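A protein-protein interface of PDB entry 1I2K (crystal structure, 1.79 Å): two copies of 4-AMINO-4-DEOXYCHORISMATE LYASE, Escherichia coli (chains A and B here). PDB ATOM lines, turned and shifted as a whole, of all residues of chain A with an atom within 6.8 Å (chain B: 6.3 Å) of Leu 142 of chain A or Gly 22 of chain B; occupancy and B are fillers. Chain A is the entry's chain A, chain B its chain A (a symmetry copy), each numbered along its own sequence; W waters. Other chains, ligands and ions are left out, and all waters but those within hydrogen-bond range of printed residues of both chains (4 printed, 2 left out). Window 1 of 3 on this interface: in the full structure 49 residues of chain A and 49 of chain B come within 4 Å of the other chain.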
ATOM      1  N   ASP A  16     -20.456 -26.355  13.780  1.00  0.00           N
ATOM      2  CA  ASP A  16     -20.069 -25.751  12.488  1.00  0.00           C
ATOM      3  C   ASP A  16     -21.282 -25.203  11.748  1.00  0.00           C
ATOM      4  O   ASP A  16     -22.340 -25.811  11.706  1.00  0.00           O
ATOM      5  CB  ASP A  16     -19.333 -26.752  11.605  1.00  0.00           C
ATOM      6  CG  ASP A  16     -18.643 -26.073  10.430  1.00  0.00           C
ATOM      7  OD1 ASP A  16     -19.281 -25.846   9.379  1.00  0.00           O
ATOM      8  OD2 ASP A  16     -17.445 -25.726  10.565  1.00  0.00           O
ATOM      9  N   ARG A  17     -21.146 -24.014  11.141  1.00  0.00           N
ATOM     10  CA  ARG A  17     -22.365 -23.399  10.574  1.00  0.00           C
ATOM     11  C   ARG A  17     -22.802 -24.078   9.293  1.00  0.00           C
ATOM     12  O   ARG A  17     -23.913 -23.835   8.795  1.00  0.00           O
ATOM     13  CB  ARG A  17     -22.118 -21.891  10.419  1.00  0.00           C
ATOM     14  CG  ARG A  17     -22.049 -21.146  11.752  1.00  0.00           C
ATOM     15  CD  ARG A  17     -21.560 -19.719  11.582  1.00  0.00           C
ATOM     16  NE  ARG A  17     -22.399 -18.909  10.667  1.00  0.00           N
ATOM     17  CZ  ARG A  17     -23.273 -18.029  11.139  1.00  0.00           C
ATOM     18  NH1 ARG A  17     -23.405 -17.877  12.465  1.00  0.00           N
ATOM     19  NH2 ARG A  17     -23.999 -17.313  10.288  1.00  0.00           N
ATOM     20  N   ALA A  18     -21.987 -24.974   8.729  1.00  0.00           N
ATOM     21  CA  ALA A  18     -22.523 -25.818   7.662  1.00  0.00           C
ATOM     22  C   ALA A  18     -23.651 -26.684   8.223  1.00  0.00           C
ATOM     23  O   ALA A  18     -24.725 -26.819   7.660  1.00  0.00           O
ATOM     24  CB  ALA A  18     -21.459 -26.705   7.044  1.00  0.00           C
ATOM     25  N   THR A  19     -23.376 -27.306   9.363  1.00  0.00           N
ATOM     26  CA  THR A  19     -24.358 -28.200   9.985  1.00  0.00           C
ATOM     27  C   THR A  19     -25.585 -27.442  10.429  1.00  0.00           C
ATOM     28  O   THR A  19     -26.693 -27.964  10.359  1.00  0.00           O
ATOM     29  CB  THR A  19     -23.688 -28.881  11.198  1.00  0.00           C
ATOM     30  OG1 THR A  19     -22.498 -29.505  10.709  1.00  0.00           O
ATOM     31  CG2 THR A  19     -24.554 -29.982  11.800  1.00  0.00           C
ATOM     32  N   GLN A  20     -25.374 -26.211  10.915  1.00  0.00           N
ATOM     33  CA  GLN A  20     -26.502 -25.506  11.513  1.00  0.00           C
ATOM     34  C   GLN A  20     -27.384 -24.771  10.514  1.00  0.00           C
ATOM     35  O   GLN A  20     -28.592 -24.640  10.730  1.00  0.00           O
ATOM     36  CB  GLN A  20     -26.045 -24.493  12.569  1.00  0.00           C
ATOM     37  CG  GLN A  20     -25.219 -25.033  13.709  1.00  0.00           C
ATOM     38  CD  GLN A  20     -26.001 -25.957  14.625  1.00  0.00           C
ATOM     39  OE1 GLN A  20     -25.355 -27.052  15.039  1.00  0.00           O
ATOM     40  NE2 GLN A  20     -27.159 -25.697  14.935  1.00  0.00           N
ATOM     41  N   PHE A  21     -26.840 -24.218   9.436  1.00  0.00           N
ATOM     42  CA  PHE A  21     -27.593 -23.289   8.609  1.00  0.00           C
ATOM     43  C   PHE A  21     -27.218 -23.521   7.153  1.00  0.00           C
ATOM     44  O   PHE A  21     -27.622 -22.728   6.303  1.00  0.00           O
ATOM     45  CB  PHE A  21     -27.286 -21.830   8.941  1.00  0.00           C
ATOM     46  CG  PHE A  21     -27.460 -21.377  10.369  1.00  0.00           C
ATOM     47  CD1 PHE A  21     -28.579 -21.707  11.110  1.00  0.00           C
ATOM     48  CD2 PHE A  21     -26.468 -20.581  10.943  1.00  0.00           C
ATOM     49  CE1 PHE A  21     -28.697 -21.268  12.420  1.00  0.00           C
ATOM     50  CE2 PHE A  21     -26.562 -20.156  12.259  1.00  0.00           C
ATOM     51  CZ  PHE A  21     -27.692 -20.500  12.976  1.00  0.00           C
ATOM     52  N   GLY A  22     -26.429 -24.561   6.856  1.00  0.00           N
ATOM     53  CA  GLY A  22     -25.943 -24.681   5.486  1.00  0.00           C
ATOM     54  C   GLY A  22     -25.107 -23.481   5.081  1.00  0.00           C
ATOM     55  O   GLY A  22     -25.138 -23.097   3.903  1.00  0.00           O
ATOM     56  N   ASP A  23     -24.375 -22.874   6.025  1.00  0.00           N
ATOM     57  CA  ASP A  23     -23.716 -21.591   5.740  1.00  0.00           C
ATOM     58  C   ASP A  23     -22.377 -21.745   5.027  1.00  0.00           C
ATOM     59  O   ASP A  23     -21.302 -21.726   5.639  1.00  0.00           O
ATOM     60  CB  ASP A  23     -23.629 -20.817   7.055  1.00  0.00           C
ATOM     61  CG  ASP A  23     -23.194 -19.378   6.939  1.00  0.00           C
ATOM     62  OD1 ASP A  23     -23.016 -18.866   5.805  1.00  0.00           O
ATOM     63  OD2 ASP A  23     -22.994 -18.735   7.992  1.00  0.00           O
ATOM     64  N   GLY A  24     -22.404 -21.936   3.704  1.00  0.00           N
ATOM     65  CA  GLY A  24     -21.195 -22.283   2.966  1.00  0.00           C
ATOM     66  C   GLY A  24     -21.439 -22.626   1.503  1.00  0.00           C
ATOM     67  O   GLY A  24     -22.544 -22.448   0.984  1.00  0.00           O
ATOM     68  N   CYS A  25     -20.390 -23.133   0.855  1.00  0.00           N
ATOM     69  CA  CYS A  25     -20.474 -23.464  -0.564  1.00  0.00           C
ATOM     70  C   CYS A  25     -19.700 -24.737  -0.866  1.00  0.00           C
ATOM     71  O   CYS A  25     -19.037 -25.280   0.036  1.00  0.00           O
ATOM     72  CB  CYS A  25     -19.975 -22.268  -1.355  1.00  0.00           C
ATOM     73  SG  CYS A  25     -18.207 -21.972  -1.085  1.00  0.00           S
ATOM     74  N   PHE A  26     -19.778 -25.254  -2.093  1.00  0.00           N
ATOM     75  CA  PHE A  26     -19.031 -26.486  -2.401  1.00  0.00           C
ATOM     76  C   PHE A  26     -18.738 -26.595  -3.895  1.00  0.00           C
ATOM     77  O   PHE A  26     -19.306 -25.805  -4.656  1.00  0.00           O
ATOM     78  CB  PHE A  26     -19.802 -27.702  -1.894  1.00  0.00           C
ATOM     79  CG  PHE A  26     -21.104 -28.064  -2.611  1.00  0.00           C
ATOM     80  CD1 PHE A  26     -22.265 -27.334  -2.431  1.00  0.00           C
ATOM     81  CD2 PHE A  26     -21.154 -29.173  -3.449  1.00  0.00           C
ATOM     82  CE1 PHE A  26     -23.446 -27.704  -3.059  1.00  0.00           C
ATOM     83  CE2 PHE A  26     -22.321 -29.545  -4.101  1.00  0.00           C
ATOM     84  CZ  PHE A  26     -23.469 -28.802  -3.906  1.00  0.00           C
ATOM     85  N   LEU A  53     -20.773 -14.700  -0.308  1.00  0.00           N
ATOM     86  CA  LEU A  53     -21.271 -15.013   1.040  1.00  0.00           C
ATOM     87  C   LEU A  53     -20.514 -14.301   2.150  1.00  0.00           C
ATOM     88  O   LEU A  53     -20.780 -14.565   3.325  1.00  0.00           O
ATOM     89  CB  LEU A  53     -21.217 -16.528   1.296  1.00  0.00           C
ATOM     90  CG  LEU A  53     -22.070 -17.356   0.329  1.00  0.00           C
ATOM     91  CD1 LEU A  53     -21.825 -18.854   0.513  1.00  0.00           C
ATOM     92  CD2 LEU A  53     -23.542 -16.990   0.501  1.00  0.00           C
ATOM     93  N   LYS A  80     -14.714 -33.789  -3.971  1.00  0.00           N
ATOM     94  CA  LYS A  80     -15.688 -32.837  -3.434  1.00  0.00           C
ATOM     95  C   LYS A  80     -15.046 -31.911  -2.411  1.00  0.00           C
ATOM     96  O   LYS A  80     -14.332 -32.404  -1.528  1.00  0.00           O
ATOM     97  CB  LYS A  80     -16.892 -33.543  -2.774  1.00  0.00           C
ATOM     98  CG  LYS A  80     -17.952 -32.560  -2.291  1.00  0.00           C
ATOM     99  CD  LYS A  80     -19.212 -33.201  -1.763  1.00  0.00           C
ATOM    100  CE  LYS A  80     -20.251 -32.136  -1.404  1.00  0.00           C
ATOM    101  NZ  LYS A  80     -21.575 -32.778  -1.109  1.00  0.00           N
ATOM    102  N   VAL A  81     -15.296 -30.601  -2.520  1.00  0.00           N
ATOM    103  CA  VAL A  81     -14.709 -29.639  -1.579  1.00  0.00           C
ATOM    104  C   VAL A  81     -15.854 -28.888  -0.909  1.00  0.00           C
ATOM    105  O   VAL A  81     -16.751 -28.396  -1.625  1.00  0.00           O
ATOM    106  CB  VAL A  81     -13.763 -28.632  -2.265  1.00  0.00           C
ATOM    107  CG1 VAL A  81     -13.251 -27.586  -1.277  1.00  0.00           C
ATOM    108  CG2 VAL A  81     -12.580 -29.331  -2.920  1.00  0.00           C
ATOM    109  N   VAL A  82     -15.855 -28.781   0.421  1.00  0.00           N
ATOM    110  CA  VAL A  82     -16.860 -27.927   1.067  1.00  0.00           C
ATOM    111  C   VAL A  82     -16.146 -26.798   1.811  1.00  0.00           C
ATOM    112  O   VAL A  82     -15.142 -27.054   2.474  1.00  0.00           O
ATOM    113  CB  VAL A  82     -17.769 -28.730   2.017  1.00  0.00           C
ATOM    114  CG1 VAL A  82     -18.613 -27.771   2.852  1.00  0.00           C
ATOM    115  CG2 VAL A  82     -18.651 -29.697   1.232  1.00  0.00           C
ATOM    116  N   ILE A  83     -16.616 -25.549   1.714  1.00  0.00           N
ATOM    117  CA  ILE A  83     -16.078 -24.486   2.581  1.00  0.00           C
ATOM    118  C   ILE A  83     -17.229 -23.915   3.400  1.00  0.00           C
ATOM    119  O   ILE A  83     -18.292 -23.602   2.830  1.00  0.00           O
ATOM    120  CB  ILE A  83     -15.392 -23.360   1.800  1.00  0.00           C
ATOM    121  CG1 ILE A  83     -14.080 -23.775   1.116  1.00  0.00           C
ATOM    122  CG2 ILE A  83     -15.162 -22.126   2.688  1.00  0.00           C
ATOM    123  CD1 ILE A  83     -13.826 -22.979  -0.158  1.00  0.00           C
ATOM    124  N   SER A  84     -17.089 -23.765   4.713  1.00  0.00           N
ATOM    125  CA  SER A  84     -18.187 -23.170   5.501  1.00  0.00           C
ATOM    126  C   SER A  84     -17.683 -21.964   6.290  1.00  0.00           C
ATOM    127  O   SER A  84     -16.462 -21.859   6.462  1.00  0.00           O
ATOM    128  CB  SER A  84     -18.804 -24.185   6.475  1.00  0.00           C
ATOM    129  OG  SER A  84     -17.989 -24.260   7.636  1.00  0.00           O
ATOM    130  N   ILE A 139     -24.668 -19.200  -7.349  1.00  0.00           N
ATOM    131  CA  ILE A 139     -23.678 -19.743  -6.434  1.00  0.00           C
ATOM    132  C   ILE A 139     -23.903 -21.207  -6.103  1.00  0.00           C
ATOM    133  O   ILE A 139     -25.039 -21.590  -5.775  1.00  0.00           O
ATOM    134  CB  ILE A 139     -23.762 -18.988  -5.078  1.00  0.00           C
ATOM    135  CG1 ILE A 139     -23.901 -17.475  -5.201  1.00  0.00           C
ATOM    136  CG2 ILE A 139     -22.573 -19.385  -4.211  1.00  0.00           C
ATOM    137  CD1 ILE A 139     -24.039 -16.757  -3.870  1.00  0.00           C
ATOM    138  N   LYS A 140     -22.879 -22.049  -6.099  1.00  0.00           N
ATOM    139  CA  LYS A 140     -23.127 -23.420  -5.622  1.00  0.00           C
ATOM    140  C   LYS A 140     -23.071 -23.499  -4.102  1.00  0.00           C
ATOM    141  O   LYS A 140     -22.129 -24.085  -3.544  1.00  0.00           O
ATOM    142  CB  LYS A 140     -22.085 -24.356  -6.233  1.00  0.00           C
ATOM    143  CG  LYS A 140     -22.457 -25.830  -6.286  1.00  0.00           C
ATOM    144  CD  LYS A 140     -21.521 -26.578  -7.236  1.00  0.00           C
ATOM    145  CE  LYS A 140     -21.818 -28.058  -7.363  1.00  0.00           C
ATOM    146  NZ  LYS A 140     -23.193 -28.359  -7.854  1.00  0.00           N
ATOM    147  N   HIS A 141     -24.041 -22.922  -3.405  1.00  0.00           N
ATOM    148  CA  HIS A 141     -24.061 -22.874  -1.945  1.00  0.00           C
ATOM    149  C   HIS A 141     -24.614 -24.157  -1.353  1.00  0.00           C
ATOM    150  O   HIS A 141     -25.095 -25.003  -2.122  1.00  0.00           O
ATOM    151  CB  HIS A 141     -24.863 -21.644  -1.472  1.00  0.00           C
ATOM    152  CG  HIS A 141     -26.274 -21.619  -1.987  1.00  0.00           C
ATOM    153  ND1 HIS A 141     -27.280 -22.432  -1.525  1.00  0.00           N
ATOM    154  CD2 HIS A 141     -26.840 -20.855  -2.961  1.00  0.00           C
ATOM    155  CE1 HIS A 141     -28.412 -22.170  -2.170  1.00  0.00           C
ATOM    156  NE2 HIS A 141     -28.160 -21.216  -3.061  1.00  0.00           N
ATOM    157  N   LEU A 142     -24.523 -24.336  -0.034  1.00  0.00           N
ATOM    158  CA  LEU A 142     -24.936 -25.570   0.639  1.00  0.00           C
ATOM    159  C   LEU A 142     -26.427 -25.677   0.912  1.00  0.00           C
ATOM    160  O   LEU A 142     -26.848 -26.732   1.402  1.00  0.00           O
ATOM    161  CB  LEU A 142     -24.175 -25.698   1.973  1.00  0.00           C
ATOM    162  CG  LEU A 142     -22.650 -25.872   1.895  1.00  0.00           C
ATOM    163  CD1 LEU A 142     -22.044 -25.818   3.306  1.00  0.00           C
ATOM    164  CD2 LEU A 142     -22.178 -27.171   1.257  1.00  0.00           C
ATOM    165  N   ASN A 143     -27.230 -24.643   0.635  1.00  0.00           N
ATOM    166  CA  ASN A 143     -28.663 -24.706   0.906  1.00  0.00           C
ATOM    167  C   ASN A 143     -29.351 -25.471  -0.213  1.00  0.00           C
ATOM    168  O   ASN A 143     -29.890 -24.851  -1.136  1.00  0.00           O
ATOM    169  CB  ASN A 143     -29.284 -23.307   1.061  1.00  0.00           C
ATOM    170  CG  ASN A 143     -29.166 -22.727   2.446  1.00  0.00           C
ATOM    171  OD1 ASN A 143     -30.020 -21.933   2.897  1.00  0.00           O
ATOM    172  ND2 ASN A 143     -28.118 -23.110   3.175  1.00  0.00           N
ATOM    173  N   ARG A 144     -29.340 -26.809  -0.152  1.00  0.00           N
ATOM    174  CA  ARG A 144     -29.818 -27.524  -1.340  1.00  0.00           C
ATOM    175  C   ARG A 144     -31.049 -28.367  -1.080  1.00  0.00           C
ATOM    176  O   ARG A 144     -31.239 -29.385  -1.757  1.00  0.00           O
ATOM    177  CB  ARG A 144     -28.667 -28.386  -1.902  1.00  0.00           C
ATOM    178  CG  ARG A 144     -27.424 -27.560  -2.172  1.00  0.00           C
ATOM    179  CD  ARG A 144     -27.278 -27.034  -3.569  1.00  0.00           C
ATOM    180  NE  ARG A 144     -28.223 -26.091  -4.130  1.00  0.00           N
ATOM    181  CZ  ARG A 144     -27.979 -24.849  -4.547  1.00  0.00           C
ATOM    182  NH1 ARG A 144     -26.781 -24.286  -4.470  1.00  0.00           N
ATOM    183  NH2 ARG A 144     -28.964 -24.119  -5.056  1.00  0.00           N
ATOM    184  N   LEU A 145     -31.869 -27.963  -0.110  1.00  0.00           N
ATOM    185  CA  LEU A 145     -33.119 -28.680   0.122  1.00  0.00           C
ATOM    186  C   LEU A 145     -33.997 -28.654  -1.109  1.00  0.00           C
ATOM    187  O   LEU A 145     -34.742 -29.598  -1.363  1.00  0.00           O
ATOM    188  CB  LEU A 145     -33.900 -28.099   1.327  1.00  0.00           C
ATOM    189  CG  LEU A 145     -33.718 -28.896   2.624  1.00  0.00           C
ATOM    190  CD1 LEU A 145     -34.328 -28.174   3.823  1.00  0.00           C
ATOM    191  CD2 LEU A 145     -34.307 -30.293   2.499  1.00  0.00           C
ATOM    192  N   ARG B  17     -26.120 -35.323   6.391  1.00  0.00           N
ATOM    193  CA  ARG B  17     -26.693 -34.466   5.331  1.00  0.00           C
ATOM    194  C   ARG B  17     -27.090 -33.102   5.854  1.00  0.00           C
ATOM    195  O   ARG B  17     -27.390 -32.187   5.071  1.00  0.00           O
ATOM    196  CB  ARG B  17     -27.847 -35.230   4.663  1.00  0.00           C
ATOM    197  CG  ARG B  17     -27.381 -36.414   3.815  1.00  0.00           C
ATOM    198  CD  ARG B  17     -28.540 -37.290   3.377  1.00  0.00           C
ATOM    199  NE  ARG B  17     -29.570 -36.566   2.595  1.00  0.00           N
ATOM    200  CZ  ARG B  17     -29.631 -36.678   1.274  1.00  0.00           C
ATOM    201  NH1 ARG B  17     -28.740 -37.453   0.636  1.00  0.00           N
ATOM    202  NH2 ARG B  17     -30.574 -36.023   0.608  1.00  0.00           N
ATOM    203  N   ALA B  18     -27.074 -32.889   7.172  1.00  0.00           N
ATOM    204  CA  ALA B  18     -27.188 -31.511   7.649  1.00  0.00           C
ATOM    205  C   ALA B  18     -25.986 -30.706   7.156  1.00  0.00           C
ATOM    206  O   ALA B  18     -26.092 -29.602   6.648  1.00  0.00           O
ATOM    207  CB  ALA B  18     -27.267 -31.433   9.162  1.00  0.00           C
ATOM    208  N   THR B  19     -24.803 -31.281   7.339  1.00  0.00           N
ATOM    209  CA  THR B  19     -23.568 -30.595   6.948  1.00  0.00           C
ATOM    210  C   THR B  19     -23.498 -30.403   5.453  1.00  0.00           C
ATOM    211  O   THR B  19     -22.984 -29.393   4.983  1.00  0.00           O
ATOM    212  CB  THR B  19     -22.372 -31.446   7.429  1.00  0.00           C
ATOM    213  OG1 THR B  19     -22.556 -31.650   8.833  1.00  0.00           O
ATOM    214  CG2 THR B  19     -21.039 -30.730   7.252  1.00  0.00           C
ATOM    215  N   GLN B  20     -23.996 -31.398   4.706  1.00  0.00           N
ATOM    216  CA  GLN B  20     -23.799 -31.338   3.263  1.00  0.00           C
ATOM    217  C   GLN B  20     -24.832 -30.500   2.523  1.00  0.00           C
ATOM    218  O   GLN B  20     -24.520 -29.896   1.493  1.00  0.00           O
ATOM    219  CB  GLN B  20     -23.789 -32.735   2.631  1.00  0.00           C
ATOM    220  CG  GLN B  20     -22.771 -33.710   3.167  1.00  0.00           C
ATOM    221  CD  GLN B  20     -21.341 -33.318   2.838  1.00  0.00           C
ATOM    222  OE1 GLN B  20     -20.450 -33.486   3.820  1.00  0.00           O
ATOM    223  NE2 GLN B  20     -21.056 -32.861   1.736  1.00  0.00           N
ATOM    224  N   PHE B  21     -26.088 -30.469   2.955  1.00  0.00           N
ATOM    225  CA  PHE B  21     -27.149 -29.908   2.134  1.00  0.00           C
ATOM    226  C   PHE B  21     -28.129 -29.179   3.040  1.00  0.00           C
ATOM    227  O   PHE B  21     -29.188 -28.771   2.562  1.00  0.00           O
ATOM    228  CB  PHE B  21     -27.928 -30.980   1.373  1.00  0.00           C
ATOM    229  CG  PHE B  21     -27.153 -31.926   0.492  1.00  0.00           C
ATOM    230  CD1 PHE B  21     -26.174 -31.481  -0.377  1.00  0.00           C
ATOM    231  CD2 PHE B  21     -27.457 -33.287   0.541  1.00  0.00           C
ATOM    232  CE1 PHE B  21     -25.487 -32.388  -1.170  1.00  0.00           C
ATOM    233  CE2 PHE B  21     -26.761 -34.207  -0.228  1.00  0.00           C
ATOM    234  CZ  PHE B  21     -25.788 -33.734  -1.088  1.00  0.00           C
ATOM    235  N   GLY B  22     -27.819 -29.042   4.335  1.00  0.00           N
ATOM    236  CA  GLY B  22     -28.833 -28.488   5.226  1.00  0.00           C
ATOM    237  C   GLY B  22     -30.084 -29.348   5.255  1.00  0.00           C
ATOM    238  O   GLY B  22     -31.186 -28.801   5.403  1.00  0.00           O
ATOM    239  N   ASP B  23     -29.942 -30.671   5.103  1.00  0.00           N
ATOM    240  CA  ASP B  23     -31.124 -31.525   4.913  1.00  0.00           C
ATOM    241  C   ASP B  23     -31.809 -31.909   6.221  1.00  0.00           C
ATOM    242  O   ASP B  23     -31.591 -32.990   6.782  1.00  0.00           O
ATOM    243  CB  ASP B  23     -30.694 -32.724   4.067  1.00  0.00           C
ATOM    244  CG  ASP B  23     -31.811 -33.602   3.564  1.00  0.00           C
ATOM    245  OD1 ASP B  23     -33.008 -33.278   3.773  1.00  0.00           O
ATOM    246  OD2 ASP B  23     -31.509 -34.658   2.968  1.00  0.00           O
ATOM    247  N   GLY B  24     -32.640 -31.013   6.765  1.00  0.00           N
ATOM    248  CA  GLY B  24     -33.190 -31.208   8.101  1.00  0.00           C
ATOM    249  C   GLY B  24     -33.978 -30.017   8.626  1.00  0.00           C
ATOM    250  O   GLY B  24     -34.252 -29.062   7.893  1.00  0.00           O
ATOM    251  N   CYS B  25     -34.326 -30.086   9.911  1.00  0.00           N
ATOM    252  CA  CYS B  25     -35.123 -29.031  10.531  1.00  0.00           C
ATOM    253  C   CYS B  25     -34.660 -28.773  11.955  1.00  0.00           C
ATOM    254  O   CYS B  25     -33.780 -29.498  12.454  1.00  0.00           O
ATOM    255  CB  CYS B  25     -36.583 -29.437  10.449  1.00  0.00           C
ATOM    256  SG  CYS B  25     -36.935 -30.896  11.464  1.00  0.00           S
ATOM    257  N   HIS B 141     -36.831 -25.241   8.580  1.00  0.00           N
ATOM    258  CA  HIS B 141     -35.798 -26.121   8.041  1.00  0.00           C
ATOM    259  C   HIS B 141     -34.413 -25.520   8.204  1.00  0.00           C
ATOM    260  O   HIS B 141     -34.320 -24.356   8.621  1.00  0.00           O
ATOM    261  CB  HIS B 141     -36.101 -26.442   6.563  1.00  0.00           C
ATOM    262  CG  HIS B 141     -36.211 -25.219   5.698  1.00  0.00           C
ATOM    263  ND1 HIS B 141     -35.140 -24.459   5.295  1.00  0.00           N
ATOM    264  CD2 HIS B 141     -37.307 -24.617   5.161  1.00  0.00           C
ATOM    265  CE1 HIS B 141     -35.554 -23.451   4.535  1.00  0.00           C
ATOM    266  NE2 HIS B 141     -36.879 -23.524   4.452  1.00  0.00           N
ATOM    267  N   LEU B 142     -33.356 -26.285   7.928  1.00  0.00           N
ATOM    268  CA  LEU B 142     -31.973 -25.848   8.136  1.00  0.00           C
ATOM    269  C   LEU B 142     -31.406 -24.981   7.023  1.00  0.00           C
ATOM    270  O   LEU B 142     -30.272 -24.512   7.181  1.00  0.00           O
ATOM    271  CB  LEU B 142     -31.071 -27.085   8.312  1.00  0.00           C
ATOM    272  CG  LEU B 142     -31.318 -27.961   9.550  1.00  0.00           C
ATOM    273  CD1 LEU B 142     -30.450 -29.226   9.479  1.00  0.00           C
ATOM    274  CD2 LEU B 142     -31.022 -27.292  10.886  1.00  0.00           C
ATOM    275  N   ASN B 143     -32.126 -24.764   5.917  1.00  0.00           N
ATOM    276  CA  ASN B 143     -31.601 -23.955   4.821  1.00  0.00           C
ATOM    277  C   ASN B 143     -31.775 -22.483   5.158  1.00  0.00           C
ATOM    278  O   ASN B 143     -32.745 -21.863   4.709  1.00  0.00           O
ATOM    279  CB  ASN B 143     -32.284 -24.283   3.481  1.00  0.00           C
ATOM    280  CG  ASN B 143     -31.683 -25.455   2.750  1.00  0.00           C
ATOM    281  OD1 ASN B 143     -31.706 -25.528   1.503  1.00  0.00           O
ATOM    282  ND2 ASN B 143     -31.111 -26.402   3.493  1.00  0.00           N
ATOM    283  N   LEU B 145     -29.559 -19.742   4.780  1.00  0.00           N
ATOM    284  CA  LEU B 145     -28.670 -18.730   4.220  1.00  0.00           C
ATOM    285  C   LEU B 145     -29.406 -17.430   3.986  1.00  0.00           C
ATOM    286  O   LEU B 145     -28.820 -16.354   4.094  1.00  0.00           O
ATOM    287  CB  LEU B 145     -28.019 -19.203   2.897  1.00  0.00           C
ATOM    288  CG  LEU B 145     -26.589 -19.730   3.064  1.00  0.00           C
ATOM    289  CD1 LEU B 145     -26.071 -20.377   1.782  1.00  0.00           C
ATOM    290  CD2 LEU B 145     -25.644 -18.626   3.513  1.00  0.00           C
HETATM  291  O   HOH W   1     -32.090 -20.061   2.479  1.00  0.00           O
HETATM  292  O   HOH W   2     -22.669 -30.309  -0.662  1.00  0.00           O
HETATM  293  O   HOH W   3     -21.497 -35.547   0.167  1.00  0.00           O
HETATM  294  O   HOH W   4     -32.826 -24.780  -0.977  1.00  0.00           O
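O of Phe 21 of chain A lies close to O of Leu 142 of chain B (3.3 Å). O of Phe 21 of chain B lies close to O of Leu 142 of chain A. The backbone NH (N) of Arg 144 of chain A lies within hydrogen-bond range of the backbone carbonyl oxygen (O) of Phe 21 of chain B, at 3.4 Å. The side-chain amide nitrogen (NE2) of Gln 20 of chain B sits close to the side-chain amino group (NZ) of Lys 80 of chain A, at 2.9 Å. The backbone carbonyl oxygen (O) of Ala 18 of chain A lies close to the backbone carbonyl oxygen (O) of Ala 18 of chain B, at 3.3 Å. OG1 of Thr 19 of chain A lies within hydrogen-bond range of OG1 of Thr 19 of chain B, 2.9 Å away. OD1 of Asn 143 of chain B sits at hydrogen-bond distance from N of Arg 144 of chain A (3.2 Å). The side-chain amide oxygen (OD1) of Asn 143 of chain A sits at hydrogen-bond distance from the backbone NH (N) of Leu 145 of chain B (2.9 Å). The backbone carbonyl oxygen (O) of Asn 143 of chain A sits close to the side-chain amide oxygen (OD1) of Asn 143 of chain B, at 3.3 Å. N of Leu 145 of chain A sits at hydrogen-bond distance from OD1 of Asn 143 of chain B (2.9 Å).
N of Asn 143 of chain A lies within hydrogen-bond range of ND1 of His 141 of chain A. The guanidinium group (NE) of Arg 17 of chain A lies within salt-bridge range of the side-chain carboxylate (OD2) of Asp 23 of chain A, at 2.7 Å. OD2 of Asp 23 of chain B lies within salt-bridge range of NE of Arg 17 of chain B, at 2.7 Å. N of Gly 22 of chain A lies within hydrogen-bond range of O of Arg 17 of chain A (3.3 Å).
Phe 21 of chain A touches Leu 142 of chain B, and with the chains exchanged Leu 142 of chain A touches Phe 21 of chain B. Asn 143 of chain A touches its own counterpart, Asn 143 of chain B. Asn 143 of chain A touches Leu 145 of chain B, and with the chains exchanged Leu 145 of chain A touches Asn 143 of chain B. Of the 25 pairs that touch across the chains among the printed residues, 21 have their exchanged pair printed and touching as well.
Printed residues of chain A that touch a printed residue of chain B: Ala 18, Thr 19, Gln 20, Phe 21, Gly 22, Asp 23, Lys 80, His 141, Leu 142, Asn 143, Arg 144 and Leu 145. Hydrophobic or aromatic side chains of chain A that line the printed part of chain B: Ala 18, His 141, Leu 142 and Leu 145. Of the 13 printed residues of chain B, 10 touch a printed residue of chain A. Printed residues of chain B that touch a printed residue of chain A: Ala 18, Thr 19, Gln 20, Phe 21, Gly 22, Asp 23, His 141, Leu 142, Asn 143 and Leu 145.
Of the printed residues of chain B, Ala 18 of chain A touches Ala 18 and Thr 19. Leu 53 of chain A touches none of the printed residues of chain B. Ser 84 of chain A touches none of the printed residues of chain B. Printed residues of chain A within 4 Å of Phe 21 of chain B: Lys 80, Leu 142, Arg 144 and Leu 145. Of the printed residues of chain A, Asp 23 of chain B touches Leu 145. The nearest residue of chain A that does not touch Gly 22 of chain B is Gly 22 of chain A (4.8 Å). The nearest printed residue of chain A that does not touch Leu 145 of chain B is Leu 53 of chain A (4.02 Å).
Water W2 lies within hydrogen-bond range of the side-chain amino group (NZ) of Lys 80 of chain A (2.7 Å) and the backbone carbonyl oxygen (O) of Gln 20 of chain B (2.9 Å). Water W1 lies within hydrogen-bond range of the side-chain amide oxygen of Asn 143 of chain A (2.8 Å), the backbone carbonyl oxygen of Asn 143 of chain B (2.9 Å) and the backbone NH of Leu 145 of chain B (3.4 Å). Water W3 lies within hydrogen-bond range of NZ of Lys 80 of chain A and NE2 of Gln 20 of chain B.
Gln 20 of chain A touches Leu 142 of chain B. Phe 21 of chain A touches Leu 145 of chain B (O to N, 3.9 Å). Gly 22 of chain A touches Leu 142 of chain B (N to O, 3.9 Å). NZ of Lys 80 of chain A touches CE1 of Phe 21 of chain B, 3.9 Å away. CD2 of Leu 142 of chain A touches O of Gln 20 of chain B, 3.6 Å away. N of Leu 145 of chain A touches O of Phe 21 of chain B, at 3.9 Å. O of Gly 22 of chain B touches CD1 of Leu 145 of chain A, at 3.6 Å. His 141 of chain B touches Leu 145 of chain A (CB to CD1, 3.7 Å).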
